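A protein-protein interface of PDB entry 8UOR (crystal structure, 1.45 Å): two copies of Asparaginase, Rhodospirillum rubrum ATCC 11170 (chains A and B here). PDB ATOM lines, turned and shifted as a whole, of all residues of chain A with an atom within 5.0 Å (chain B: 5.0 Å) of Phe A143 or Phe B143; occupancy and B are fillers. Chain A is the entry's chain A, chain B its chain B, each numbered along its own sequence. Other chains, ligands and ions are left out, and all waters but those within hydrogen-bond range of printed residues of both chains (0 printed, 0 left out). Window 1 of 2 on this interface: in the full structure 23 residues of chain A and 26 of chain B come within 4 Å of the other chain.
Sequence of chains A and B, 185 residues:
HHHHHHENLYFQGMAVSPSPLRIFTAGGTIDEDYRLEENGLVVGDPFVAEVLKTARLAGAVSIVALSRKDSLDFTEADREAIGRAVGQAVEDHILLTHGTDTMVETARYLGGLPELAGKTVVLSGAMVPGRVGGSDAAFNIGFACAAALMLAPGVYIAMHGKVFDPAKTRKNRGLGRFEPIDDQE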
ATOM      1  N   PHE A 139       1.729  12.601 -26.312  1.00  0.00           N
ATOM      2  CA  PHE A 139       2.372  13.735 -25.658  1.00  0.00           C
ATOM      3  C   PHE A 139       2.212  13.637 -24.152  1.00  0.00           C
ATOM      4  O   PHE A 139       3.127  13.848 -23.383  1.00  0.00           O
ATOM      5  CB  PHE A 139       1.755  15.028 -26.222  1.00  0.00           C
ATOM      6  CG  PHE A 139       2.271  16.242 -25.477  1.00  0.00           C
ATOM      7  CD1 PHE A 139       1.643  16.698 -24.352  1.00  0.00           C
ATOM      8  CD2 PHE A 139       3.353  16.930 -25.937  1.00  0.00           C
ATOM      9  CE1 PHE A 139       2.136  17.787 -23.628  1.00  0.00           C
ATOM     10  CE2 PHE A 139       3.869  18.022 -25.234  1.00  0.00           C
ATOM     11  CZ  PHE A 139       3.247  18.432 -24.076  1.00  0.00           C
ATOM     12  N   ASN A 140       0.972  13.365 -23.739  1.00  0.00           N
ATOM     13  CA  ASN A 140       0.693  13.355 -22.296  1.00  0.00           C
ATOM     14  C   ASN A 140       1.518  12.275 -21.580  1.00  0.00           C
ATOM     15  O   ASN A 140       1.956  12.536 -20.463  1.00  0.00           O
ATOM     16  CB  ASN A 140      -0.772  13.107 -22.005  1.00  0.00           C
ATOM     17  CG  ASN A 140      -1.748  14.173 -22.405  1.00  0.00           C
ATOM     18  OD1 ASN A 140      -1.285  15.286 -22.705  1.00  0.00           O
ATOM     19  ND2 ASN A 140      -3.036  13.825 -22.440  1.00  0.00           N
ATOM     20  N   ILE A 141       1.704  11.134 -22.226  1.00  0.00           N
ATOM     21  CA  ILE A 141       2.500  10.083 -21.574  1.00  0.00           C
ATOM     22  C   ILE A 141       3.960  10.531 -21.490  1.00  0.00           C
ATOM     23  O   ILE A 141       4.585  10.325 -20.453  1.00  0.00           O
ATOM     24  CB  ILE A 141       2.326   8.790 -22.378  1.00  0.00           C
ATOM     25  CG1 ILE A 141       0.903   8.204 -22.222  1.00  0.00           C
ATOM     26  CG2 ILE A 141       3.417   7.793 -21.983  1.00  0.00           C
ATOM     27  CD1 ILE A 141       0.403   8.052 -20.807  1.00  0.00           C
ATOM     28  N   GLY A 142       4.518  11.097 -22.549  1.00  0.00           N
ATOM     29  CA  GLY A 142       5.887  11.607 -22.435  1.00  0.00           C
ATOM     30  C   GLY A 142       6.070  12.609 -21.328  1.00  0.00           C
ATOM     31  O   GLY A 142       7.025  12.526 -20.525  1.00  0.00           O
ATOM     32  N   PHE A 143       5.170  13.616 -21.329  1.00  0.00           N
ATOM     33  CA  PHE A 143       5.234  14.659 -20.307  1.00  0.00           C
ATOM     34  C   PHE A 143       5.088  14.093 -18.901  1.00  0.00           C
ATOM     35  O   PHE A 143       5.817  14.490 -18.009  1.00  0.00           O
ATOM     36  CB  PHE A 143       4.119  15.636 -20.657  1.00  0.00           C
ATOM     37  CG  PHE A 143       4.197  16.906 -19.840  1.00  0.00           C
ATOM     38  CD1 PHE A 143       3.640  16.962 -18.573  1.00  0.00           C
ATOM     39  CD2 PHE A 143       4.811  18.051 -20.341  1.00  0.00           C
ATOM     40  CE1 PHE A 143       3.732  18.096 -17.789  1.00  0.00           C
ATOM     41  CE2 PHE A 143       4.964  19.172 -19.521  1.00  0.00           C
ATOM     42  CZ  PHE A 143       4.410  19.179 -18.263  1.00  0.00           C
ATOM     43  N   ALA A 144       4.145  13.145 -18.720  1.00  0.00           N
ATOM     44  CA  ALA A 144       3.864  12.620 -17.386  1.00  0.00           C
ATOM     45  C   ALA A 144       4.993  11.690 -16.907  1.00  0.00           C
ATOM     46  O   ALA A 144       5.252  11.661 -15.711  1.00  0.00           O
ATOM     47  CB  ALA A 144       2.532  11.851 -17.363  1.00  0.00           C
ATOM     48  N   CYS A 145       5.633  10.956 -17.832  1.00  0.00           N
ATOM     49  CA  CYS A 145       6.788  10.152 -17.441  1.00  0.00           C
ATOM     50  C   CYS A 145       7.887  11.066 -16.881  1.00  0.00           C
ATOM     51  O   CYS A 145       8.484  10.774 -15.862  1.00  0.00           O
ATOM     52  CB  CYS A 145       7.322   9.301 -18.593  1.00  0.00           C
ATOM     53  SG  CYS A 145       6.303   7.873 -19.003  1.00  0.00           S
ATOM     54  N   ALA A 146       8.203  12.130 -17.627  1.00  0.00           N
ATOM     55  CA  ALA A 146       9.211  13.113 -17.176  1.00  0.00           C
ATOM     56  C   ALA A 146       8.789  13.690 -15.842  1.00  0.00           C
ATOM     57  O   ALA A 146       9.640  13.779 -14.928  1.00  0.00           O
ATOM     58  CB  ALA A 146       9.471  14.138 -18.197  1.00  0.00           C
ATOM     59  N   ALA A 147       7.534  14.079 -15.710  1.00  0.00           N
ATOM     60  CA  ALA A 147       7.054  14.703 -14.453  1.00  0.00           C
ATOM     61  C   ALA A 147       7.288  13.722 -13.288  1.00  0.00           C
ATOM     62  O   ALA A 147       7.732  14.130 -12.187  1.00  0.00           O
ATOM     63  CB  ALA A 147       5.615  15.101 -14.553  1.00  0.00           C
ATOM     64  N   LEU A 149       9.444  11.447 -12.908  1.00  0.00           N
ATOM     65  CA  LEU A 149      10.894  11.349 -12.627  1.00  0.00           C
ATOM     66  C   LEU A 149      11.467  12.607 -11.985  1.00  0.00           C
ATOM     67  O   LEU A 149      12.389  12.460 -11.170  1.00  0.00           O
ATOM     68  CB  LEU A 149      11.680  11.082 -13.913  1.00  0.00           C
ATOM     69  CG  LEU A 149      11.381   9.722 -14.547  1.00  0.00           C
ATOM     70  CD1 LEU A 149      11.987   9.652 -15.937  1.00  0.00           C
ATOM     71  CD2 LEU A 149      11.867   8.540 -13.668  1.00  0.00           C
ATOM     72  N   MET A 150      10.926  13.779 -12.334  1.00  0.00           N
ATOM     73  CA  MET A 150      11.634  15.053 -12.007  1.00  0.00           C
ATOM     74  C   MET A 150      10.955  15.792 -10.844  1.00  0.00           C
ATOM     75  O   MET A 150      11.646  16.544 -10.151  1.00  0.00           O
ATOM     76  CB  MET A 150      11.591  15.953 -13.240  1.00  0.00           C
ATOM     77  CG  MET A 150      12.448  15.391 -14.369  1.00  0.00           C
ATOM     78  SD  MET A 150      12.189  16.298 -15.891  1.00  0.00           S
ATOM     79  CE  MET A 150      12.785  15.049 -17.022  1.00  0.00           C
ATOM     80  N   ALA A 158      -0.803  15.596 -14.308  1.00  0.00           N
ATOM     81  CA  ALA A 158      -0.059  16.176 -15.434  1.00  0.00           C
ATOM     82  C   ALA A 158      -0.882  16.075 -16.709  1.00  0.00           C
ATOM     83  O   ALA A 158      -1.270  14.996 -17.119  1.00  0.00           O
ATOM     84  CB  ALA A 158       1.248  15.453 -15.641  1.00  0.00           C
ATOM     85  N   GLY A 161       0.205  19.806 -20.760  1.00  0.00           N
ATOM     86  CA  GLY A 161       1.605  20.241 -20.671  1.00  0.00           C
ATOM     87  C   GLY A 161       1.923  21.048 -19.426  1.00  0.00           C
ATOM     88  O   GLY A 161       2.845  21.874 -19.487  1.00  0.00           O
ATOM     89  N   LYS A 162       1.219  20.802 -18.328  1.00  0.00           N
ATOM     90  CA  LYS A 162       1.536  21.439 -17.050  1.00  0.00           C
ATOM     91  C   LYS A 162       1.169  20.494 -15.906  1.00  0.00           C
ATOM     92  O   LYS A 162       0.564  19.419 -16.126  1.00  0.00           O
ATOM     93  CB  LYS A 162       0.861  22.789 -17.016  1.00  0.00           C
ATOM     94  CG  LYS A 162      -0.618  22.654 -16.938  1.00  0.00           C
ATOM     95  CD  LYS A 162      -1.278  23.957 -16.482  1.00  0.00           C
ATOM     96  CE  LYS A 162      -1.267  24.000 -15.001  1.00  0.00           C
ATOM     97  NZ  LYS A 162      -1.952  25.210 -14.515  1.00  0.00           N
ATOM     98  N   VAL A 163       1.579  20.911 -14.752  1.00  0.00           N
ATOM     99  CA  VAL A 163       1.365  20.189 -13.488  1.00  0.00           C
ATOM    100  C   VAL A 163       0.298  20.899 -12.663  1.00  0.00           C
ATOM    101  O   VAL A 163       0.462  22.076 -12.349  1.00  0.00           O
ATOM    102  CB  VAL A 163       2.703  20.029 -12.765  1.00  0.00           C
ATOM    103  CG1 VAL A 163       2.516  19.292 -11.452  1.00  0.00           C
ATOM    104  CG2 VAL A 163       3.736  19.321 -13.638  1.00  0.00           C
ATOM    105  N   PHE B 139       6.224  11.034 -28.047  1.00  0.00           N
ATOM    106  CA  PHE B 139       6.657  10.799 -26.666  1.00  0.00           C
ATOM    107  C   PHE B 139       7.853  11.673 -26.324  1.00  0.00           C
ATOM    108  O   PHE B 139       7.888  12.317 -25.270  1.00  0.00           O
ATOM    109  CB  PHE B 139       7.077   9.318 -26.526  1.00  0.00           C
ATOM    110  CG  PHE B 139       7.706   8.998 -25.194  1.00  0.00           C
ATOM    111  CD1 PHE B 139       9.080   9.147 -24.985  1.00  0.00           C
ATOM    112  CD2 PHE B 139       6.936   8.604 -24.123  1.00  0.00           C
ATOM    113  CE1 PHE B 139       9.640   8.867 -23.749  1.00  0.00           C
ATOM    114  CE2 PHE B 139       7.485   8.376 -22.886  1.00  0.00           C
ATOM    115  CZ  PHE B 139       8.843   8.482 -22.704  1.00  0.00           C
ATOM    116  N   ASN B 140       8.833  11.752 -27.255  1.00  0.00           N
ATOM    117  CA  ASN B 140      10.023  12.567 -27.008  1.00  0.00           C
ATOM    118  C   ASN B 140       9.679  14.055 -26.788  1.00  0.00           C
ATOM    119  O   ASN B 140      10.279  14.698 -25.954  1.00  0.00           O
ATOM    120  CB  ASN B 140      11.063  12.422 -28.105  1.00  0.00           C
ATOM    121  CG  ASN B 140      11.715  11.054 -28.236  1.00  0.00           C
ATOM    122  OD1 ASN B 140      11.590  10.270 -27.288  1.00  0.00           O
ATOM    123  ND2 ASN B 140      12.364  10.861 -29.359  1.00  0.00           N
ATOM    124  N   ILE B 141       8.717  14.538 -27.564  1.00  0.00           N
ATOM    125  CA  ILE B 141       8.333  15.939 -27.408  1.00  0.00           C
ATOM    126  C   ILE B 141       7.671  16.176 -26.060  1.00  0.00           C
ATOM    127  O   ILE B 141       7.995  17.155 -25.385  1.00  0.00           O
ATOM    128  CB  ILE B 141       7.438  16.361 -28.592  1.00  0.00           C
ATOM    129  CG1 ILE B 141       8.261  16.410 -29.878  1.00  0.00           C
ATOM    130  CG2 ILE B 141       6.757  17.659 -28.341  1.00  0.00           C
ATOM    131  CD1 ILE B 141       7.465  16.250 -31.167  1.00  0.00           C
ATOM    132  N   GLY B 142       6.765  15.316 -25.637  1.00  0.00           N
ATOM    133  CA  GLY B 142       6.151  15.461 -24.323  1.00  0.00           C
ATOM    134  C   GLY B 142       7.200  15.446 -23.216  1.00  0.00           C
ATOM    135  O   GLY B 142       7.202  16.271 -22.308  1.00  0.00           O
ATOM    136  N   PHE B 143       8.088  14.441 -23.266  1.00  0.00           N
ATOM    137  CA  PHE B 143       9.125  14.266 -22.262  1.00  0.00           C
ATOM    138  C   PHE B 143      10.037  15.506 -22.218  1.00  0.00           C
ATOM    139  O   PHE B 143      10.356  15.997 -21.131  1.00  0.00           O
ATOM    140  CB  PHE B 143       9.881  12.984 -22.565  1.00  0.00           C
ATOM    141  CG  PHE B 143      10.811  12.557 -21.444  1.00  0.00           C
ATOM    142  CD1 PHE B 143      12.056  13.141 -21.343  1.00  0.00           C
ATOM    143  CD2 PHE B 143      10.456  11.554 -20.537  1.00  0.00           C
ATOM    144  CE1 PHE B 143      12.935  12.732 -20.338  1.00  0.00           C
ATOM    145  CE2 PHE B 143      11.302  11.215 -19.512  1.00  0.00           C
ATOM    146  CZ  PHE B 143      12.512  11.846 -19.399  1.00  0.00           C
ATOM    147  N   ALA B 144      10.422  15.967 -23.390  1.00  0.00           N
ATOM    148  CA  ALA B 144      11.362  17.115 -23.465  1.00  0.00           C
ATOM    149  C   ALA B 144      10.704  18.456 -23.069  1.00  0.00           C
ATOM    150  O   ALA B 144      11.418  19.283 -22.510  1.00  0.00           O
ATOM    151  CB  ALA B 144      11.915  17.195 -24.820  1.00  0.00           C
ATOM    152  N   CYS B 145       9.434  18.607 -23.305  1.00  0.00           N
ATOM    153  CA  CYS B 145       8.737  19.803 -22.846  1.00  0.00           C
ATOM    154  C   CYS B 145       8.709  19.838 -21.328  1.00  0.00           C
ATOM    155  O   CYS B 145       9.020  20.855 -20.712  1.00  0.00           O
ATOM    156  CB  CYS B 145       7.310  19.865 -23.368  1.00  0.00           C
ATOM    157  SG  CYS B 145       7.159  20.386 -25.088  1.00  0.00           S
ATOM    158  N   ALA B 146       8.373  18.706 -20.669  1.00  0.00           N
ATOM    159  CA  ALA B 146       8.437  18.588 -19.198  1.00  0.00           C
ATOM    160  C   ALA B 146       9.850  18.893 -18.731  1.00  0.00           C
ATOM    161  O   ALA B 146      10.029  19.646 -17.769  1.00  0.00           O
ATOM    162  CB  ALA B 146       7.913  17.237 -18.789  1.00  0.00           C
ATOM    163  N   ALA B 147      10.847  18.297 -19.381  1.00  0.00           N
ATOM    164  CA  ALA B 147      12.259  18.496 -18.976  1.00  0.00           C
ATOM    165  C   ALA B 147      12.627  19.999 -19.055  1.00  0.00           C
ATOM    166  O   ALA B 147      13.258  20.550 -18.132  1.00  0.00           O
ATOM    167  CB  ALA B 147      13.191  17.657 -19.797  1.00  0.00           C
ATOM    168  N   LEU B 149      10.753  22.517 -18.712  1.00  0.00           N
ATOM    169  CA  LEU B 149       9.997  23.238 -17.659  1.00  0.00           C
ATOM    170  C   LEU B 149      10.580  22.958 -16.284  1.00  0.00           C
ATOM    171  O   LEU B 149      10.587  23.887 -15.429  1.00  0.00           O
ATOM    172  CB  LEU B 149       8.510  22.934 -17.677  1.00  0.00           C
ATOM    173  CG  LEU B 149       7.766  23.446 -18.886  1.00  0.00           C
ATOM    174  CD1 LEU B 149       6.361  22.924 -18.803  1.00  0.00           C
ATOM    175  CD2 LEU B 149       7.813  24.964 -19.010  1.00  0.00           C
ATOM    176  N   MET B 150      11.055  21.742 -16.065  1.00  0.00           N
ATOM    177  CA  MET B 150      11.296  21.247 -14.705  1.00  0.00           C
ATOM    178  C   MET B 150      12.771  21.185 -14.299  1.00  0.00           C
ATOM    179  O   MET B 150      13.041  21.260 -13.057  1.00  0.00           O
ATOM    180  CB  MET B 150      10.690  19.844 -14.520  1.00  0.00           C
ATOM    181  CG  MET B 150       9.179  19.874 -14.637  1.00  0.00           C
ATOM    182  SD  MET B 150       8.504  18.223 -14.657  1.00  0.00           S
ATOM    183  CE  MET B 150       6.899  18.610 -15.341  1.00  0.00           C
ATOM    184  N   ALA B 158      17.386  15.242 -24.020  1.00  0.00           N
ATOM    185  CA  ALA B 158      16.269  14.403 -23.511  1.00  0.00           C
ATOM    186  C   ALA B 158      15.870  13.449 -24.616  1.00  0.00           C
ATOM    187  O   ALA B 158      15.303  13.870 -25.616  1.00  0.00           O
ATOM    188  CB  ALA B 158      15.123  15.258 -23.064  1.00  0.00           C
ATOM    189  N   GLY B 161      13.558   8.531 -22.998  1.00  0.00           N
ATOM    190  CA  GLY B 161      12.915   8.606 -21.683  1.00  0.00           C
ATOM    191  C   GLY B 161      13.877   8.924 -20.557  1.00  0.00           C
ATOM    192  O   GLY B 161      13.568   8.593 -19.415  1.00  0.00           O
ATOM    193  N   LYS B 162      15.018   9.584 -20.857  1.00  0.00           N
ATOM    194  CA  LYS B 162      15.956  10.011 -19.799  1.00  0.00           C
ATOM    195  C   LYS B 162      16.646  11.308 -20.226  1.00  0.00           C
ATOM    196  O   LYS B 162      16.552  11.701 -21.414  1.00  0.00           O
ATOM    197  CB  LYS B 162      16.888   8.890 -19.483  1.00  0.00           C
ATOM    198  CG  LYS B 162      17.747   8.514 -20.592  1.00  0.00           C
ATOM    199  CD  LYS B 162      18.941   7.613 -20.067  1.00  0.00           C
ATOM    200  CE  LYS B 162      20.002   8.510 -19.551  1.00  0.00           C
ATOM    201  NZ  LYS B 162      21.087   7.741 -18.958  1.00  0.00           N
ATOM    202  N   VAL B 163      17.318  11.877 -19.246  1.00  0.00           N
ATOM    203  CA  VAL B 163      18.056  13.127 -19.383  1.00  0.00           C
ATOM    204  C   VAL B 163      19.552  12.805 -19.408  1.00  0.00           C
ATOM    205  O   VAL B 163      20.087  12.150 -18.490  1.00  0.00           O
ATOM    206  CB  VAL B 163      17.689  14.073 -18.255  1.00  0.00           C
ATOM    207  CG1 VAL B 163      18.522  15.351 -18.333  1.00  0.00           C
ATOM    208  CG2 VAL B 163      16.177  14.354 -18.248  1.00  0.00           C
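The backbone carbonyl oxygen (O) of Gly B142 lies close to the backbone NH (N) of Phe A143.
Among the printed residues, pairs that only touch across the chains: Phe A139 with Gly B142 (3.5 Å), Gly A142 with Phe B139 (3.5 Å), Gly A142 with Gly B142 (3.6 Å), Gly A142 with Phe B143 (3.2 Å), Phe A143 with Phe B143 (3.6 Å), Phe A143 with Ala B146 (3.5 Å), Phe A143 with Met B150 (3.9 Å), Ala A146 with Phe B143 (3.6 Å), Ala A146 with Ala B146 (3.5 Å), Ala A147 with Met B150 (3.8 Å), Leu A149 with Phe B143 (3.96 Å), Leu A149 with Gly B161 (3.96 Å), Met A150 with Phe B143 (3.998 Å), Met A150 with Ala B147 (3.8 Å), Met A150 with Val B163 (3.7 Å), Gly A161 with Leu B149 (3.7 Å) and Val A163 with Met B150 (3.7 Å).
Printed residues of chain A within 4 Å of Phe B139: Gly A142.
Of the printed residues of chain A, Gly B142 touches Phe A139, Gly A142 and Phe A143.
Of the printed residues of chain A, Ala B147 touches Met A150 (3.8 Å).
Of the printed residues of chain A, Met B150 touches Phe A143, Ala A147 and Val A163.
Printed residues of chain A that touch a printed residue of chain B: Phe A139, Gly A142, Phe A143, Ala A146, Ala A147, Leu A149, Met A150, Gly A161 and Val A163.
Hydrophobic or aromatic side chains of chain B within 4 Å of the printed part of chain A: Phe B139, Phe B143, Ala B146, Ala B147, Leu B149, Met B150 and Val B163.
Phe A139 touches Gly B142, and with the chains exchanged Gly A142 touches Phe B139.
Phe B143 touches its own counterpart, Phe A143.
Ala A146 touches its own counterpart, Ala B146.
Ala A147 touches Met B150, and with the chains exchanged Met A150 touches Ala B147.
Positions printed for both chains: 139, 140, 141, 142, 143, 144, 145, 146, 147, 149, 150, 158, 161, 162 and 163.
Of the 18 pairs that touch across the chains among the printed residues, 17 have their exchanged pair printed and touching as well.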
